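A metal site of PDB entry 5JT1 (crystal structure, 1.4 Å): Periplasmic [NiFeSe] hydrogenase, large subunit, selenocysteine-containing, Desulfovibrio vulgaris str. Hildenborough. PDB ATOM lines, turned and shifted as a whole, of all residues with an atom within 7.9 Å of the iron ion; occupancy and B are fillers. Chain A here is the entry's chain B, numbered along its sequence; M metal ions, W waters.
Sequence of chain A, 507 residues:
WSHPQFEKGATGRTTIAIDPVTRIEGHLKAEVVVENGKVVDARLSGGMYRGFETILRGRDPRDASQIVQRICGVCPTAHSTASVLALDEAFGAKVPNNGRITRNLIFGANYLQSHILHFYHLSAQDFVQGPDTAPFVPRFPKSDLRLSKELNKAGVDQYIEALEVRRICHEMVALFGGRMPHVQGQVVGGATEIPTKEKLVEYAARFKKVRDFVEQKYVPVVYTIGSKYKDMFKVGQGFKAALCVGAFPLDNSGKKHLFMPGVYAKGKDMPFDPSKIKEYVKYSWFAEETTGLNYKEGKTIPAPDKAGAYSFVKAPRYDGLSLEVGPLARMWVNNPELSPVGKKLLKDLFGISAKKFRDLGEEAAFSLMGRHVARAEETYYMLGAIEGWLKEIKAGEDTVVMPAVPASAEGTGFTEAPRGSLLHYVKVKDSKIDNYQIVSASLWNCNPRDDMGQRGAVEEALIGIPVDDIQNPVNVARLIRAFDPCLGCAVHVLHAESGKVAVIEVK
Water W1 lies within hydrogen-bond range of the side-chain carboxylate of Glu 279 (2.6 Å), the side-chain amide oxygen of Gln 437 (2.7 Å) and the side-chain amino group of Lys 314 (3.1 Å).
Water W3 bridges OE1 of Glu 53 (2.6 Å) and NZ of Lys 314 (3.2 Å).
NE2 of His 492 binds the iron ion, 2.1 Å away.
Water W2 binds the iron ion.
Water W1 binds the iron ion.
OE2 of Glu 53 binds the iron ion (2.2 Å).
The iron ion is bound by the backbone carbonyl oxygen (O) of Ile 438.
The iron ion is bound by water W3 (2.2 Å).
The iron ion has six donor atoms within binding distance.
ND1 of His 492 is in hydrogen-bond range of O of Cys 489 (2.8 Å).
The side-chain amide oxygen (OE1) of Gln 437 sits close to the side-chain carboxylate (OE2) of Glu 53.
OE1 of Glu 53 lies within hydrogen-bond range of OG1 of Thr 300, 2.7 Å away.
Of the 19 residues printed, 3 come within 4 Å of the iron ion.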
ATOM      1  N   GLU A  53     -15.554  13.848  23.808  1.00  0.00           N
ATOM      2  CA  GLU A  53     -15.122  14.933  22.917  1.00  0.00           C
ATOM      3  C   GLU A  53     -15.248  16.297  23.598  1.00  0.00           C
ATOM      4  O   GLU A  53     -14.509  17.226  23.252  1.00  0.00           O
ATOM      5  CB  GLU A  53     -15.902  14.898  21.593  1.00  0.00           C
ATOM      6  CG  GLU A  53     -15.543  13.665  20.770  1.00  0.00           C
ATOM      7  CD  GLU A  53     -16.654  13.138  19.829  1.00  0.00           C
ATOM      8  OE1 GLU A  53     -17.861  13.370  20.124  1.00  0.00           O
ATOM      9  OE2 GLU A  53     -16.296  12.479  18.799  1.00  0.00           O
ATOM     10  N   GLU A 279     -20.828  13.136   9.498  1.00  0.00           N
ATOM     11  CA  GLU A 279     -21.643  12.545  10.564  1.00  0.00           C
ATOM     12  C   GLU A 279     -22.988  13.256  10.657  1.00  0.00           C
ATOM     13  O   GLU A 279     -23.046  14.455  10.941  1.00  0.00           O
ATOM     14  CB  GLU A 279     -20.932  12.569  11.926  1.00  0.00           C
ATOM     15  CG  GLU A 279     -19.684  11.688  11.972  1.00  0.00           C
ATOM     16  CD  GLU A 279     -19.085  11.575  13.361  1.00  0.00           C
ATOM     17  OE1 GLU A 279     -18.355  12.485  13.789  1.00  0.00           O
ATOM     18  OE2 GLU A 279     -19.355  10.560  14.029  1.00  0.00           O
ATOM     19  N   PHE A 286     -28.457  14.497  19.407  1.00  0.00           N
ATOM     20  CA  PHE A 286     -27.569  15.664  19.327  1.00  0.00           C
ATOM     21  C   PHE A 286     -28.306  16.815  18.640  1.00  0.00           C
ATOM     22  O   PHE A 286     -29.249  16.598  17.886  1.00  0.00           O
ATOM     23  CB  PHE A 286     -26.274  15.319  18.588  1.00  0.00           C
ATOM     24  CG  PHE A 286     -25.520  14.226  19.264  1.00  0.00           C
ATOM     25  CD1 PHE A 286     -24.735  14.504  20.379  1.00  0.00           C
ATOM     26  CD2 PHE A 286     -25.669  12.905  18.883  1.00  0.00           C
ATOM     27  CE1 PHE A 286     -24.089  13.470  21.069  1.00  0.00           C
ATOM     28  CE2 PHE A 286     -25.032  11.893  19.566  1.00  0.00           C
ATOM     29  CZ  PHE A 286     -24.246  12.174  20.664  1.00  0.00           C
ATOM     30  N   TYR A 295     -15.416  15.452  10.326  1.00  0.00           N
ATOM     31  CA  TYR A 295     -14.812  15.417  11.666  1.00  0.00           C
ATOM     32  C   TYR A 295     -13.892  16.612  11.941  1.00  0.00           C
ATOM     33  O   TYR A 295     -13.759  17.022  13.096  1.00  0.00           O
ATOM     34  CB  TYR A 295     -14.076  14.073  11.901  1.00  0.00           C
ATOM     35  CG  TYR A 295     -12.997  13.817  10.878  1.00  0.00           C
ATOM     36  CD1 TYR A 295     -11.738  14.390  11.014  1.00  0.00           C
ATOM     37  CD2 TYR A 295     -13.251  13.088   9.718  1.00  0.00           C
ATOM     38  CE1 TYR A 295     -10.737  14.189  10.064  1.00  0.00           C
ATOM     39  CE2 TYR A 295     -12.264  12.895   8.752  1.00  0.00           C
ATOM     40  CZ  TYR A 295     -11.016  13.452   8.920  1.00  0.00           C
ATOM     41  OH  TYR A 295     -10.055  13.270   7.937  1.00  0.00           O
ATOM     42  N   LYS A 299     -18.782  18.609  15.930  1.00  0.00           N
ATOM     43  CA  LYS A 299     -19.358  19.185  17.142  1.00  0.00           C
ATOM     44  C   LYS A 299     -20.154  18.105  17.844  1.00  0.00           C
ATOM     45  O   LYS A 299     -20.773  17.245  17.193  1.00  0.00           O
ATOM     46  CB  LYS A 299     -20.296  20.349  16.811  1.00  0.00           C
ATOM     47  CG  LYS A 299     -19.595  21.548  16.212  1.00  0.00           C
ATOM     48  CD  LYS A 299     -20.572  22.691  16.011  1.00  0.00           C
ATOM     49  CE  LYS A 299     -19.844  23.991  15.652  1.00  0.00           C
ATOM     50  NZ  LYS A 299     -18.892  24.413  16.737  1.00  0.00           N
ATOM     51  N   THR A 300     -20.186  18.186  19.174  1.00  0.00           N
ATOM     52  CA  THR A 300     -20.873  17.191  20.003  1.00  0.00           C
ATOM     53  C   THR A 300     -21.696  17.921  21.055  1.00  0.00           C
ATOM     54  O   THR A 300     -21.169  18.357  22.088  1.00  0.00           O
ATOM     55  CB  THR A 300     -19.867  16.216  20.593  1.00  0.00           C
ATOM     56  OG1 THR A 300     -19.110  15.643  19.524  1.00  0.00           O
ATOM     57  CG2 THR A 300     -20.580  15.109  21.387  1.00  0.00           C
ATOM     58  N   PHE A 312     -27.601   7.459  20.903  1.00  0.00           N
ATOM     59  CA  PHE A 312     -26.451   8.334  21.138  1.00  0.00           C
ATOM     60  C   PHE A 312     -25.314   8.127  20.133  1.00  0.00           C
ATOM     61  O   PHE A 312     -24.279   8.791  20.233  1.00  0.00           O
ATOM     62  CB  PHE A 312     -25.927   8.217  22.571  1.00  0.00           C
ATOM     63  CG  PHE A 312     -26.834   8.808  23.615  1.00  0.00           C
ATOM     64  CD1 PHE A 312     -27.063  10.177  23.645  1.00  0.00           C
ATOM     65  CD2 PHE A 312     -27.434   8.000  24.586  1.00  0.00           C
ATOM     66  CE1 PHE A 312     -27.897  10.746  24.634  1.00  0.00           C
ATOM     67  CE2 PHE A 312     -28.257   8.556  25.579  1.00  0.00           C
ATOM     68  CZ  PHE A 312     -28.496   9.919  25.589  1.00  0.00           C
ATOM     69  N   LYS A 314     -23.845   8.751  16.549  1.00  0.00           N
ATOM     70  CA  LYS A 314     -24.036   9.542  15.330  1.00  0.00           C
ATOM     71  C   LYS A 314     -24.083   8.594  14.115  1.00  0.00           C
ATOM     72  O   LYS A 314     -23.792   7.402  14.212  1.00  0.00           O
ATOM     73  CB  LYS A 314     -22.887  10.548  15.156  1.00  0.00           C
ATOM     74  CG  LYS A 314     -22.781  11.664  16.230  1.00  0.00           C
ATOM     75  CD  LYS A 314     -21.621  12.592  15.940  1.00  0.00           C
ATOM     76  CE  LYS A 314     -21.470  13.709  16.992  1.00  0.00           C
ATOM     77  NZ  LYS A 314     -20.160  14.429  16.859  1.00  0.00           N
ATOM     78  N   LEU A 423     -10.564   6.826  13.640  1.00  0.00           N
ATOM     79  CA  LEU A 423      -9.753   8.036  13.507  1.00  0.00           C
ATOM     80  C   LEU A 423     -10.039   8.984  14.669  1.00  0.00           C
ATOM     81  O   LEU A 423     -11.160   9.059  15.195  1.00  0.00           O
ATOM     82  CB  LEU A 423      -9.942   8.720  12.155  1.00  0.00           C
ATOM     83  CG  LEU A 423     -11.270   9.415  11.974  1.00  0.00           C
ATOM     84  CD1 LEU A 423     -11.230  10.859  12.458  1.00  0.00           C
ATOM     85  CD2 LEU A 423     -11.688   9.368  10.494  1.00  0.00           C
ATOM     86  N   TYR A 436     -11.591  17.989  19.764  1.00  0.00           N
ATOM     87  CA  TYR A 436     -11.150  16.600  19.620  1.00  0.00           C
ATOM     88  C   TYR A 436     -12.346  15.818  19.113  1.00  0.00           C
ATOM     89  O   TYR A 436     -13.386  15.780  19.789  1.00  0.00           O
ATOM     90  CB  TYR A 436     -10.655  16.035  20.948  1.00  0.00           C
ATOM     91  CG  TYR A 436      -9.692  14.870  20.821  1.00  0.00           C
ATOM     92  CD1 TYR A 436     -10.142  13.600  20.470  1.00  0.00           C
ATOM     93  CD2 TYR A 436      -8.325  15.041  21.062  1.00  0.00           C
ATOM     94  CE1 TYR A 436      -9.260  12.534  20.383  1.00  0.00           C
ATOM     95  CE2 TYR A 436      -7.441  13.983  20.971  1.00  0.00           C
ATOM     96  CZ  TYR A 436      -7.906  12.740  20.619  1.00  0.00           C
ATOM     97  OH  TYR A 436      -7.008  11.678  20.528  1.00  0.00           O
ATOM     98  N   GLN A 437     -12.217  15.195  17.947  1.00  0.00           N
ATOM     99  CA  GLN A 437     -13.319  14.439  17.354  1.00  0.00           C
ATOM    100  C   GLN A 437     -12.908  13.012  17.060  1.00  0.00           C
ATOM    101  O   GLN A 437     -11.820  12.746  16.519  1.00  0.00           O
ATOM    102  CB  GLN A 437     -13.872  15.154  16.096  1.00  0.00           C
ATOM    103  CG  GLN A 437     -14.687  16.379  16.447  1.00  0.00           C
ATOM    104  CD  GLN A 437     -16.001  16.056  17.126  1.00  0.00           C
ATOM    105  OE1 GLN A 437     -16.685  15.122  16.771  1.00  0.00           O
ATOM    106  NE2 GLN A 437     -16.363  16.856  18.114  1.00  0.00           N
ATOM    107  N   ILE A 438     -13.808  12.085  17.412  1.00  0.00           N
ATOM    108  CA  ILE A 438     -13.581  10.640  17.314  1.00  0.00           C
ATOM    109  C   ILE A 438     -14.641  10.032  16.400  1.00  0.00           C
ATOM    110  O   ILE A 438     -15.842  10.240  16.595  1.00  0.00           O
ATOM    111  CB  ILE A 438     -13.568  10.006  18.718  1.00  0.00           C
ATOM    112  CG1 ILE A 438     -12.365  10.558  19.497  1.00  0.00           C
ATOM    113  CG2 ILE A 438     -13.497   8.478  18.616  1.00  0.00           C
ATOM    114  CD1 ILE A 438     -12.485  10.422  20.992  1.00  0.00           C
ATOM    115  N   VAL A 439     -14.183   9.255  15.420  1.00  0.00           N
ATOM    116  CA  VAL A 439     -15.029   8.499  14.512  1.00  0.00           C
ATOM    117  C   VAL A 439     -14.525   7.050  14.599  1.00  0.00           C
ATOM    118  O   VAL A 439     -13.446   6.730  14.058  1.00  0.00           O
ATOM    119  CB  VAL A 439     -14.938   9.063  13.068  1.00  0.00           C
ATOM    120  CG1 VAL A 439     -15.801   8.302  12.087  1.00  0.00           C
ATOM    121  CG2 VAL A 439     -15.282  10.572  13.033  1.00  0.00           C
ATOM    122  N   SER A 440     -15.292   6.176  15.274  1.00  0.00           N
ATOM    123  CA  SER A 440     -14.824   4.856  15.722  1.00  0.00           C
ATOM    124  C   SER A 440     -15.456   3.708  14.930  1.00  0.00           C
ATOM    125  O   SER A 440     -16.370   3.875  14.113  1.00  0.00           O
ATOM    126  CB  SER A 440     -15.146   4.710  17.196  1.00  0.00           C
ATOM    127  OG  SER A 440     -16.548   4.743  17.308  1.00  0.00           O
ATOM    128  N   LEU A 443     -19.117   2.795  15.715  1.00  0.00           N
ATOM    129  CA  LEU A 443     -19.867   3.893  15.129  1.00  0.00           C
ATOM    130  C   LEU A 443     -20.293   3.562  13.691  1.00  0.00           C
ATOM    131  O   LEU A 443     -21.466   3.687  13.323  1.00  0.00           O
ATOM    132  CB  LEU A 443     -19.018   5.166  15.182  1.00  0.00           C
ATOM    133  CG  LEU A 443     -19.491   6.374  14.386  1.00  0.00           C
ATOM    134  CD1 LEU A 443     -20.716   7.024  14.989  1.00  0.00           C
ATOM    135  CD2 LEU A 443     -18.352   7.371  14.210  1.00  0.00           C
ATOM    136  N   CYS A 489     -17.301   2.491  22.436  1.00  0.00           N
ATOM    137  CA  CYS A 489     -16.631   3.121  21.291  1.00  0.00           C
ATOM    138  C   CYS A 489     -17.608   3.845  20.391  1.00  0.00           C
ATOM    139  O   CYS A 489     -17.311   4.938  19.887  1.00  0.00           O
ATOM    140  CB  CYS A 489     -15.909   2.077  20.460  1.00  0.00           C
ATOM    141  SG  CYS A 489     -14.415   1.475  21.220  1.00  0.00           S
ATOM    142  N   ALA A 490     -18.754   3.240  20.104  1.00  0.00           N
ATOM    143  CA  ALA A 490     -19.681   3.860  19.155  1.00  0.00           C
ATOM    144  C   ALA A 490     -20.130   5.246  19.611  1.00  0.00           C
ATOM    145  O   ALA A 490     -20.287   6.147  18.781  1.00  0.00           O
ATOM    146  CB  ALA A 490     -20.891   2.954  18.965  1.00  0.00           C
ATOM    147  N   VAL A 491     -20.389   5.410  20.909  1.00  0.00           N
ATOM    148  CA  VAL A 491     -20.927   6.659  21.458  1.00  0.00           C
ATOM    149  C   VAL A 491     -19.837   7.577  22.000  1.00  0.00           C
ATOM    150  O   VAL A 491     -19.880   8.799  21.770  1.00  0.00           O
ATOM    151  CB  VAL A 491     -21.976   6.373  22.554  1.00  0.00           C
ATOM    152  CG1 VAL A 491     -22.494   7.691  23.118  1.00  0.00           C
ATOM    153  CG2 VAL A 491     -23.118   5.529  22.019  1.00  0.00           C
ATOM    154  N   HIS A 492     -18.887   7.032  22.753  1.00  0.00           N
ATOM    155  CA  HIS A 492     -17.864   7.808  23.441  1.00  0.00           C
ATOM    156  C   HIS A 492     -18.464   9.007  24.166  1.00  0.00           C
ATOM    157  O   HIS A 492     -19.466   8.841  24.906  1.00  0.00           O
ATOM    158  CB  HIS A 492     -16.642   8.167  22.536  1.00  0.00           C
ATOM    159  CG  HIS A 492     -16.968   8.609  21.141  1.00  0.00           C
ATOM    160  ND1 HIS A 492     -17.278   7.726  20.132  1.00  0.00           N
ATOM    161  CD2 HIS A 492     -16.999   9.847  20.579  1.00  0.00           C
ATOM    162  CE1 HIS A 492     -17.511   8.391  19.009  1.00  0.00           C
ATOM    163  NE2 HIS A 492     -17.350   9.691  19.250  1.00  0.00           N
HETATM  164 FE    FE M   1     -17.539  11.103  17.704  1.00  0.00          FE
HETATM  165  O   HOH W   1     -17.707  12.679  16.256  1.00  0.00           O
HETATM  166  O   HOH W   2     -18.776   9.882  16.505  1.00  0.00           O
HETATM  167  O   HOH W   3     -19.382  11.903  18.635  1.00  0.00           O
